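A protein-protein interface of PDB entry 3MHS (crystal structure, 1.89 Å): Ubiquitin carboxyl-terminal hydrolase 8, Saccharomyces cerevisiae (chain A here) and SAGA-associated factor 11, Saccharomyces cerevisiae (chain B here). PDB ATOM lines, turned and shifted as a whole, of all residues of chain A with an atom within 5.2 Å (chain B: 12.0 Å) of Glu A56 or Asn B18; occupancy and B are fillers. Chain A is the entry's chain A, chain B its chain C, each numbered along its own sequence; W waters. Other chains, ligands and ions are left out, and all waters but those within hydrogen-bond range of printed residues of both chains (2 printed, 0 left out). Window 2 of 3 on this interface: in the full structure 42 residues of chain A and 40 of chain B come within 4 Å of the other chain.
Of chain B, only Asn B18 comes within 4 Å of Glu A56. Printed residues of chain A within 4 Å of Asn B18: Glu A56, Ile A57, Asn A58 and Ser A59. Lys A50 touches none of the printed residues of chain B. Cys A54 touches none of the printed residues of chain B. Of chain B, only Asn B18 (3.1 Å), Leu B19 (3.8 Å) and Thr B22 (3.1 Å) come within 4 Å of Asn A58. Ser A59 touches just one residue of chain B: Asn B18. Gly A60 touches just these residues of chain B: Thr B21 (3.9 Å), Thr B22 (3.2 Å) and Gln B25 (3.3 Å). Printed residues of chain B within 4 Å of Asn A75: Thr B21 (2.9 Å) and Gln B25 (2.9 Å). Printed residues of chain A within 4 Å of Thr B22: Asn A58 and Gly A60. Of the printed residues of chain A, Gln B25 touches Gly A60 (3.3 Å) and Asn A75 (2.9 Å). Printed residues of chain A within 4 Å of Thr B21: Gly A60 and Asn A75. Asn B17 touches none of the printed residues of chain A. Leu B20 touches none of the printed residues of chain A. The nearest residue of chain B that does not touch Glu A56 is Gly B14 (5.7 Å). The nearest printed residue of chain A that does not touch Thr B21 is Asn A58 (4.7 Å).
N of Cys A51 sits at hydrogen-bond distance from O of Glu A56 (2.9 Å). The backbone NH of Asn A75 lies within hydrogen-bond range of the backbone carbonyl oxygen of Ser A59 (2.9 Å). The side-chain amide oxygen (OD1) of Asn A75 sits at hydrogen-bond distance from the backbone NH (N) of Gly A60, at 3.4 Å. The backbone carbonyl oxygen of Asn B17 lies within hydrogen-bond range of the side-chain hydroxyl of Thr B21, at 2.9 Å. The backbone carbonyl oxygen (O) of Asn B18 lies within hydrogen-bond range of the side-chain hydroxyl (OG1) of Thr B22 (2.8 Å). The backbone carbonyl oxygen (O) of Thr B21 sits close to the side-chain amide nitrogen (NE2) of Gln B25, at 3.3 Å.
Water W1 lies within hydrogen-bond range of OG of Ser A59 (2.8 Å) and ND2 of Asn B18 (2.8 Å). Water W2 lies within hydrogen-bond range of ND2 of Asn A75 (3.0 Å) and NE2 of Gln B25 (3.4 Å).
Printed residues of chain B that touch a printed residue of chain A: Asn B18, Leu B19, Thr B21, Thr B22 and Gln B25. Hydrophobic or aromatic side chains of chain B within 4 Å of the printed part of chain A: Leu B19. Of the 12 printed residues of chain A, 6 touch a printed residue of chain B. Among the printed residues, no Asp or Glu carboxylate lies within 4 Å of a Lys or Arg side-chain nitrogen of the other chain.
Among the printed residues, merely in contact across the chains: Gly A60 with Gln B25, Asn A58 with Leu B19, Ser A59 with Asn B18 and Gly A60 with Thr B21.
The side-chain carboxylate (OE2) of Glu A56 lies close to the side-chain amide oxygen (OD1) of Asn B18 (2.9 Å). O of Ile A57 lies close to OD1 of Asn B18, 3.2 Å away. OG1 of Thr B22 lies within hydrogen-bond range of O of Asn A58 (3.1 Å). The backbone carbonyl oxygen (O) of Gly A60 lies within hydrogen-bond range of the side-chain hydroxyl (OG1) of Thr B22 (3.2 Å). The side-chain amide oxygen of Asn A75 is in hydrogen-bond range of the side-chain hydroxyl of Thr B21 (2.9 Å). NE2 of Gln B25 sits close to ND2 of Asn A75. The backbone carbonyl oxygen (O) of Asn B18 sits close to the backbone carbonyl oxygen (O) of Asn A58.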
ATOM      1  N   MET A  49      19.151  24.951  10.072  1.00  0.00           N
ATOM      2  CA  MET A  49      20.449  24.949   9.418  1.00  0.00           C
ATOM      3  C   MET A  49      21.577  25.508  10.291  1.00  0.00           C
ATOM      4  O   MET A  49      22.666  25.815   9.807  1.00  0.00           O
ATOM      5  CB  MET A  49      20.379  25.653   8.091  1.00  0.00           C
ATOM      6  CG  MET A  49      19.512  24.882   7.082  1.00  0.00           C
ATOM      7  SD  MET A  49      19.157  25.860   5.611  1.00  0.00           S
ATOM      8  CE  MET A  49      18.078  24.716   4.720  1.00  0.00           C
ATOM      9  N   LYS A  50      21.288  25.588  11.574  1.00  0.00           N
ATOM     10  CA  LYS A  50      22.228  26.064  12.567  1.00  0.00           C
ATOM     11  C   LYS A  50      22.717  24.905  13.418  1.00  0.00           C
ATOM     12  O   LYS A  50      21.920  24.267  14.100  1.00  0.00           O
ATOM     13  CB  LYS A  50      21.559  27.085  13.479  1.00  0.00           C
ATOM     14  CG  LYS A  50      22.521  27.749  14.423  1.00  0.00           C
ATOM     15  CD  LYS A  50      21.793  28.480  15.515  1.00  0.00           C
ATOM     16  CE  LYS A  50      21.333  29.825  15.083  1.00  0.00           C
ATOM     17  NZ  LYS A  50      21.130  30.691  16.310  1.00  0.00           N
ATOM     18  N   CYS A  51      24.032  24.673  13.434  1.00  0.00           N
ATOM     19  CA  CYS A  51      24.600  23.563  14.225  1.00  0.00           C
ATOM     20  C   CYS A  51      24.483  23.791  15.728  1.00  0.00           C
ATOM     21  O   CYS A  51      24.831  24.849  16.243  1.00  0.00           O
ATOM     22  CB  CYS A  51      26.058  23.312  13.855  1.00  0.00           C
ATOM     23  SG  CYS A  51      26.918  21.960  14.828  1.00  0.00           S
ATOM     24  N   CYS A  54      28.551  23.989  17.103  1.00  0.00           N
ATOM     25  CA  CYS A  54      29.419  25.101  16.701  1.00  0.00           C
ATOM     26  C   CYS A  54      28.625  26.371  16.383  1.00  0.00           C
ATOM     27  O   CYS A  54      29.194  27.464  16.258  1.00  0.00           O
ATOM     28  CB  CYS A  54      30.287  24.701  15.503  1.00  0.00           C
ATOM     29  SG  CYS A  54      29.395  24.279  13.949  1.00  0.00           S
ATOM     30  N   HIS A  55      27.310  26.212  16.230  1.00  0.00           N
ATOM     31  CA  HIS A  55      26.395  27.325  15.981  1.00  0.00           C
ATOM     32  C   HIS A  55      26.583  28.004  14.631  1.00  0.00           C
ATOM     33  O   HIS A  55      26.012  29.069  14.371  1.00  0.00           O
ATOM     34  CB  HIS A  55      26.510  28.346  17.099  1.00  0.00           C
ATOM     35  CG  HIS A  55      26.538  27.737  18.465  1.00  0.00           C
ATOM     36  ND1 HIS A  55      25.413  27.225  19.071  1.00  0.00           N
ATOM     37  CD2 HIS A  55      27.546  27.596  19.359  1.00  0.00           C
ATOM     38  CE1 HIS A  55      25.727  26.792  20.280  1.00  0.00           C
ATOM     39  NE2 HIS A  55      27.017  26.999  20.477  1.00  0.00           N
ATOM     40  N   GLU A  56      27.334  27.373  13.740  1.00  0.00           N
ATOM     41  CA  GLU A  56      27.468  27.898  12.392  1.00  0.00           C
ATOM     42  C   GLU A  56      26.207  27.612  11.564  1.00  0.00           C
ATOM     43  O   GLU A  56      25.512  26.605  11.778  1.00  0.00           O
ATOM     44  CB  GLU A  56      28.697  27.343  11.688  1.00  0.00           C
ATOM     45  CG  GLU A  56      30.015  27.903  12.221  1.00  0.00           C
ATOM     46  CD  GLU A  56      31.201  27.486  11.381  1.00  0.00           C
ATOM     47  OE1 GLU A  56      32.165  26.948  11.955  1.00  0.00           O
ATOM     48  OE2 GLU A  56      31.162  27.662  10.138  1.00  0.00           O
ATOM     49  N   ILE A  57      25.918  28.516  10.637  1.00  0.00           N
ATOM     50  CA  ILE A  57      24.852  28.301   9.657  1.00  0.00           C
ATOM     51  C   ILE A  57      25.497  27.650   8.452  1.00  0.00           C
ATOM     52  O   ILE A  57      26.527  28.125   7.972  1.00  0.00           O
ATOM     53  CB  ILE A  57      24.171  29.618   9.211  1.00  0.00           C
ATOM     54  CG1 ILE A  57      23.698  30.458  10.411  1.00  0.00           C
ATOM     55  CG2 ILE A  57      22.988  29.324   8.238  1.00  0.00           C
ATOM     56  CD1 ILE A  57      22.774  29.761  11.376  1.00  0.00           C
ATOM     57  N   ASN A  58      24.876  26.585   7.948  1.00  0.00           N
ATOM     58  CA  ASN A  58      25.330  25.921   6.728  1.00  0.00           C
ATOM     59  C   ASN A  58      26.794  25.412   6.821  1.00  0.00           C
ATOM     60  O   ASN A  58      27.575  25.587   5.881  1.00  0.00           O
ATOM     61  CB  ASN A  58      25.212  26.851   5.517  1.00  0.00           C
ATOM     62  CG  ASN A  58      23.766  27.120   5.082  1.00  0.00           C
ATOM     63  OD1 ASN A  58      23.483  28.183   4.532  1.00  0.00           O
ATOM     64  ND2 ASN A  58      22.876  26.154   5.277  1.00  0.00           N
ATOM     65  N   SER A  59      27.151  24.802   7.947  1.00  0.00           N
ATOM     66  CA  SER A  59      28.456  24.109   8.093  1.00  0.00           C
ATOM     67  C   SER A  59      28.363  22.755   7.389  1.00  0.00           C
ATOM     68  O   SER A  59      28.443  21.670   8.001  1.00  0.00           O
ATOM     69  CB  SER A  59      28.820  23.953   9.559  1.00  0.00           C
ATOM     70  OG  SER A  59      30.183  23.602   9.725  1.00  0.00           O
ATOM     71  N   GLY A  60      28.239  22.845   6.073  1.00  0.00           N
ATOM     72  CA  GLY A  60      27.772  21.745   5.264  1.00  0.00           C
ATOM     73  C   GLY A  60      26.299  21.492   5.550  1.00  0.00           C
ATOM     74  O   GLY A  60      25.628  22.321   6.163  1.00  0.00           O
ATOM     75  N   ASN A  75      30.272  19.382   8.161  1.00  0.00           N
ATOM     76  CA  ASN A  75      31.666  19.801   7.986  1.00  0.00           C
ATOM     77  C   ASN A  75      32.560  19.593   9.215  1.00  0.00           C
ATOM     78  O   ASN A  75      33.733  19.196   9.077  1.00  0.00           O
ATOM     79  CB  ASN A  75      31.743  21.247   7.465  1.00  0.00           C
ATOM     80  CG  ASN A  75      31.333  21.366   5.986  1.00  0.00           C
ATOM     81  OD1 ASN A  75      31.488  22.419   5.364  1.00  0.00           O
ATOM     82  ND2 ASN A  75      30.856  20.281   5.419  1.00  0.00           N
ATOM     83  N   HIS A  76      32.026  19.850  10.408  1.00  0.00           N
ATOM     84  CA  HIS A  76      32.785  19.639  11.632  1.00  0.00           C
ATOM     85  C   HIS A  76      32.395  18.337  12.344  1.00  0.00           C
ATOM     86  O   HIS A  76      32.707  18.166  13.521  1.00  0.00           O
ATOM     87  CB  HIS A  76      32.623  20.825  12.600  1.00  0.00           C
ATOM     88  CG  HIS A  76      33.043  22.142  12.025  1.00  0.00           C
ATOM     89  ND1 HIS A  76      34.236  22.315  11.355  1.00  0.00           N
ATOM     90  CD2 HIS A  76      32.432  23.351  12.023  1.00  0.00           C
ATOM     91  CE1 HIS A  76      34.337  23.573  10.962  1.00  0.00           C
ATOM     92  NE2 HIS A  76      33.255  24.222  11.355  1.00  0.00           N
ATOM     93  N   ILE B   6      42.259  36.630  11.543  1.00  0.00           N
ATOM     94  CA  ILE B   6      40.934  36.674  10.951  1.00  0.00           C
ATOM     95  C   ILE B   6      40.722  38.016  10.255  1.00  0.00           C
ATOM     96  O   ILE B   6      40.966  39.086  10.832  1.00  0.00           O
ATOM     97  CB  ILE B   6      39.817  36.372  11.992  1.00  0.00           C
ATOM     98  CG1 ILE B   6      39.629  37.544  12.974  1.00  0.00           C
ATOM     99  CG2 ILE B   6      40.157  35.083  12.765  1.00  0.00           C
ATOM    100  CD1 ILE B   6      38.171  37.757  13.408  1.00  0.00           C
ATOM    101  N   ILE B   8      38.235  40.090   6.948  1.00  0.00           N
ATOM    102  CA  ILE B   8      37.075  40.087   6.062  1.00  0.00           C
ATOM    103  C   ILE B   8      37.304  39.050   4.951  1.00  0.00           C
ATOM    104  O   ILE B   8      36.436  38.221   4.699  1.00  0.00           O
ATOM    105  CB  ILE B   8      36.799  41.490   5.471  1.00  0.00           C
ATOM    106  CG1 ILE B   8      36.551  42.521   6.585  1.00  0.00           C
ATOM    107  CG2 ILE B   8      35.574  41.474   4.551  1.00  0.00           C
ATOM    108  CD1 ILE B   8      35.180  42.462   7.210  1.00  0.00           C
ATOM    109  N   ASP B   9      38.472  39.060   4.311  1.00  0.00           N
ATOM    110  CA  ASP B   9      38.772  38.053   3.285  1.00  0.00           C
ATOM    111  C   ASP B   9      38.664  36.596   3.795  1.00  0.00           C
ATOM    112  O   ASP B   9      38.093  35.729   3.106  1.00  0.00           O
ATOM    113  CB  ASP B   9      40.148  38.297   2.664  1.00  0.00           C
ATOM    114  CG  ASP B   9      40.133  39.394   1.608  1.00  0.00           C
ATOM    115  OD1 ASP B   9      39.188  40.212   1.586  1.00  0.00           O
ATOM    116  OD2 ASP B   9      41.084  39.438   0.798  1.00  0.00           O
ATOM    117  N   SER B  10      39.207  36.324   4.985  1.00  0.00           N
ATOM    118  CA  SER B  10      39.182  34.967   5.558  1.00  0.00           C
ATOM    119  C   SER B  10      37.766  34.555   5.952  1.00  0.00           C
ATOM    120  O   SER B  10      37.309  33.471   5.575  1.00  0.00           O
ATOM    121  CB  SER B  10      40.135  34.830   6.766  1.00  0.00           C
ATOM    122  OG  SER B  10      39.613  35.429   7.948  1.00  0.00           O
ATOM    123  N   ILE B  11      37.076  35.409   6.702  1.00  0.00           N
ATOM    124  CA  ILE B  11      35.713  35.100   7.120  1.00  0.00           C
ATOM    125  C   ILE B  11      34.775  34.970   5.915  1.00  0.00           C
ATOM    126  O   ILE B  11      33.899  34.119   5.898  1.00  0.00           O
ATOM    127  CB  ILE B  11      35.128  36.156   8.065  1.00  0.00           C
ATOM    128  CG1 ILE B  11      35.635  35.941   9.485  1.00  0.00           C
ATOM    129  CG2 ILE B  11      33.617  36.042   8.064  1.00  0.00           C
ATOM    130  CD1 ILE B  11      35.015  36.883  10.491  1.00  0.00           C
ATOM    131  N   SER B  12      34.977  35.815   4.913  1.00  0.00           N
ATOM    132  CA  SER B  12      34.164  35.789   3.710  1.00  0.00           C
ATOM    133  C   SER B  12      34.384  34.489   2.957  1.00  0.00           C
ATOM    134  O   SER B  12      33.427  33.889   2.461  1.00  0.00           O
ATOM    135  CB  SER B  12      34.518  36.969   2.827  1.00  0.00           C
ATOM    136  OG  SER B  12      34.135  38.152   3.477  1.00  0.00           O
ATOM    137  N   ASN B  13      35.641  34.051   2.900  1.00  0.00           N
ATOM    138  CA  ASN B  13      35.993  32.790   2.255  1.00  0.00           C
ATOM    139  C   ASN B  13      35.307  31.642   2.986  1.00  0.00           C
ATOM    140  O   ASN B  13      34.896  30.667   2.364  1.00  0.00           O
ATOM    141  CB  ASN B  13      37.515  32.561   2.235  1.00  0.00           C
ATOM    142  CG  ASN B  13      38.254  33.530   1.310  1.00  0.00           C
ATOM    143  OD1 ASN B  13      37.962  33.620   0.117  1.00  0.00           O
ATOM    144  ND2 ASN B  13      39.250  34.233   1.861  1.00  0.00           N
ATOM    145  N   GLY B  14      35.194  31.772   4.308  1.00  0.00           N
ATOM    146  CA  GLY B  14      34.563  30.753   5.137  1.00  0.00           C
ATOM    147  C   GLY B  14      33.056  30.731   4.918  1.00  0.00           C
ATOM    148  O   GLY B  14      32.436  29.678   4.929  1.00  0.00           O
ATOM    149  N   ILE B  15      32.469  31.905   4.747  1.00  0.00           N
ATOM    150  CA  ILE B  15      31.044  31.994   4.467  1.00  0.00           C
ATOM    151  C   ILE B  15      30.776  31.356   3.120  1.00  0.00           C
ATOM    152  O   ILE B  15      29.896  30.524   3.018  1.00  0.00           O
ATOM    153  CB  ILE B  15      30.537  33.436   4.560  1.00  0.00           C
ATOM    154  CG1 ILE B  15      30.456  33.827   6.044  1.00  0.00           C
ATOM    155  CG2 ILE B  15      29.152  33.578   3.829  1.00  0.00           C
ATOM    156  CD1 ILE B  15      30.321  35.330   6.324  1.00  0.00           C
ATOM    157  N   LEU B  16      31.578  31.683   2.111  1.00  0.00           N
ATOM    158  CA  LEU B  16      31.424  31.092   0.781  1.00  0.00           C
ATOM    159  C   LEU B  16      31.656  29.593   0.835  1.00  0.00           C
ATOM    160  O   LEU B  16      30.892  28.829   0.256  1.00  0.00           O
ATOM    161  CB  LEU B  16      32.370  31.735  -0.236  1.00  0.00           C
ATOM    162  CG  LEU B  16      32.331  31.200  -1.677  1.00  0.00           C
ATOM    163  CD1 LEU B  16      30.992  31.485  -2.333  1.00  0.00           C
ATOM    164  CD2 LEU B  16      33.483  31.764  -2.531  1.00  0.00           C
ATOM    165  N   ASN B  17      32.681  29.152   1.568  1.00  0.00           N
ATOM    166  CA  ASN B  17      32.897  27.726   1.692  1.00  0.00           C
ATOM    167  C   ASN B  17      31.700  27.047   2.390  1.00  0.00           C
ATOM    168  O   ASN B  17      31.269  25.977   1.987  1.00  0.00           O
ATOM    169  CB  ASN B  17      34.232  27.405   2.396  1.00  0.00           C
ATOM    170  CG  ASN B  17      34.604  25.952   2.261  1.00  0.00           C
ATOM    171  OD1 ASN B  17      34.416  25.173   3.188  1.00  0.00           O
ATOM    172  ND2 ASN B  17      35.007  25.556   1.059  1.00  0.00           N
ATOM    173  N   ASN B  18      31.116  27.675   3.400  1.00  0.00           N
ATOM    174  CA  ASN B  18      29.937  27.077   4.024  1.00  0.00           C
ATOM    175  C   ASN B  18      28.780  26.905   2.991  1.00  0.00           C
ATOM    176  O   ASN B  18      28.172  25.836   2.855  1.00  0.00           O
ATOM    177  CB  ASN B  18      29.490  27.908   5.228  1.00  0.00           C
ATOM    178  CG  ASN B  18      30.222  27.542   6.497  1.00  0.00           C
ATOM    179  OD1 ASN B  18      29.721  27.748   7.608  1.00  0.00           O
ATOM    180  ND2 ASN B  18      31.409  26.971   6.338  1.00  0.00           N
ATOM    181  N   LEU B  19      28.560  27.939   2.202  1.00  0.00           N
ATOM    182  CA  LEU B  19      27.466  27.925   1.223  1.00  0.00           C
ATOM    183  C   LEU B  19      27.704  26.898   0.134  1.00  0.00           C
ATOM    184  O   LEU B  19      26.805  26.134  -0.197  1.00  0.00           O
ATOM    185  CB  LEU B  19      27.318  29.319   0.615  1.00  0.00           C
ATOM    186  CG  LEU B  19      26.736  30.380   1.550  1.00  0.00           C
ATOM    187  CD1 LEU B  19      26.952  31.768   0.981  1.00  0.00           C
ATOM    188  CD2 LEU B  19      25.223  30.135   1.747  1.00  0.00           C
ATOM    189  N   LEU B  20      28.924  26.849  -0.396  1.00  0.00           N
ATOM    190  CA  LEU B  20      29.236  25.941  -1.496  1.00  0.00           C
ATOM    191  C   LEU B  20      29.216  24.467  -1.059  1.00  0.00           C
ATOM    192  O   LEU B  20      28.716  23.633  -1.781  1.00  0.00           O
ATOM    193  CB  LEU B  20      30.607  26.263  -2.112  1.00  0.00           C
ATOM    194  CG  LEU B  20      30.737  27.536  -2.947  1.00  0.00           C
ATOM    195  CD1 LEU B  20      32.257  27.828  -3.237  1.00  0.00           C
ATOM    196  CD2 LEU B  20      29.895  27.439  -4.229  1.00  0.00           C
ATOM    197  N   THR B  21      29.792  24.139   0.099  1.00  0.00           N
ATOM    198  CA  THR B  21      29.827  22.733   0.534  1.00  0.00           C
ATOM    199  C   THR B  21      28.426  22.199   0.890  1.00  0.00           C
ATOM    200  O   THR B  21      28.120  21.041   0.643  1.00  0.00           O
ATOM    201  CB  THR B  21      30.795  22.502   1.723  1.00  0.00           C
ATOM    202  OG1 THR B  21      30.405  23.310   2.839  1.00  0.00           O
ATOM    203  CG2 THR B  21      32.245  22.803   1.323  1.00  0.00           C
ATOM    204  N   THR B  22      27.580  23.052   1.459  1.00  0.00           N
ATOM    205  CA  THR B  22      26.168  22.713   1.689  1.00  0.00           C
ATOM    206  C   THR B  22      25.430  22.373   0.402  1.00  0.00           C
ATOM    207  O   THR B  22      24.726  21.362   0.338  1.00  0.00           O
ATOM    208  CB  THR B  22      25.415  23.839   2.371  1.00  0.00           C
ATOM    209  OG1 THR B  22      26.058  24.169   3.602  1.00  0.00           O
ATOM    210  CG2 THR B  22      23.976  23.441   2.636  1.00  0.00           C
ATOM    211  N   LEU B  23      25.568  23.237  -0.602  1.00  0.00           N
ATOM    212  CA  LEU B  23      24.954  23.016  -1.890  1.00  0.00           C
ATOM    213  C   LEU B  23      25.475  21.752  -2.553  1.00  0.00           C
ATOM    214  O   LEU B  23      24.692  20.969  -3.079  1.00  0.00           O
ATOM    215  CB  LEU B  23      25.180  24.231  -2.798  1.00  0.00           C
ATOM    216  CG  LEU B  23      24.555  24.221  -4.192  1.00  0.00           C
ATOM    217  CD1 LEU B  23      23.030  24.023  -4.122  1.00  0.00           C
ATOM    218  CD2 LEU B  23      24.928  25.544  -4.917  1.00  0.00           C
ATOM    219  N   ILE B  24      26.789  21.547  -2.512  1.00  0.00           N
ATOM    220  CA  ILE B  24      27.394  20.374  -3.107  1.00  0.00           C
ATOM    221  C   ILE B  24      26.821  19.124  -2.423  1.00  0.00           C
ATOM    222  O   ILE B  24      26.346  18.188  -3.081  1.00  0.00           O
ATOM    223  CB  ILE B  24      28.933  20.414  -2.949  1.00  0.00           C
ATOM    224  CG1 ILE B  24      29.539  21.422  -3.934  1.00  0.00           C
ATOM    225  CG2 ILE B  24      29.504  19.030  -3.166  1.00  0.00           C
ATOM    226  CD1 ILE B  24      31.012  21.780  -3.673  1.00  0.00           C
ATOM    227  N   GLN B  25      26.784  19.172  -1.102  1.00  0.00           N
ATOM    228  CA  GLN B  25      26.313  18.071  -0.296  1.00  0.00           C
ATOM    229  C   GLN B  25      24.822  17.764  -0.546  1.00  0.00           C
ATOM    230  O   GLN B  25      24.413  16.600  -0.513  1.00  0.00           O
ATOM    231  CB  GLN B  25      26.608  18.362   1.175  1.00  0.00           C
ATOM    232  CG  GLN B  25      28.124  18.173   1.507  1.00  0.00           C
ATOM    233  CD  GLN B  25      28.538  18.751   2.834  1.00  0.00           C
ATOM    234  OE1 GLN B  25      27.769  18.744   3.805  1.00  0.00           O
ATOM    235  NE2 GLN B  25      29.766  19.254   2.898  1.00  0.00           N
ATOM    236  N   ASP B  26      24.031  18.807  -0.801  1.00  0.00           N
ATOM    237  CA  ASP B  26      22.627  18.669  -1.148  1.00  0.00           C
ATOM    238  C   ASP B  26      22.488  17.965  -2.482  1.00  0.00           C
ATOM    239  O   ASP B  26      21.781  16.960  -2.586  1.00  0.00           O
ATOM    240  CB  ASP B  26      21.987  20.041  -1.213  1.00  0.00           C
ATOM    241  CG  ASP B  26      20.487  20.008  -1.518  1.00  0.00           C
ATOM    242  OD1 ASP B  26      19.799  19.000  -1.272  1.00  0.00           O
ATOM    243  OD2 ASP B  26      19.997  21.041  -1.974  1.00  0.00           O
ATOM    244  N   ILE B  27      23.196  18.478  -3.482  1.00  0.00           N
ATOM    245  CA  ILE B  27      23.178  17.925  -4.821  1.00  0.00           C
ATOM    246  C   ILE B  27      23.623  16.476  -4.799  1.00  0.00           C
ATOM    247  O   ILE B  27      22.952  15.599  -5.371  1.00  0.00           O
ATOM    248  CB  ILE B  27      24.096  18.721  -5.780  1.00  0.00           C
ATOM    249  CG1 ILE B  27      23.543  20.143  -6.000  1.00  0.00           C
ATOM    250  CG2 ILE B  27      24.231  17.976  -7.111  1.00  0.00           C
ATOM    251  CD1 ILE B  27      24.566  21.059  -6.598  1.00  0.00           C
HETATM  252  O   HOH W   1      32.016  24.818   8.074  1.00  0.00           O
HETATM  253  O   HOH W   2      33.074  19.666   3.435  1.00  0.00           O
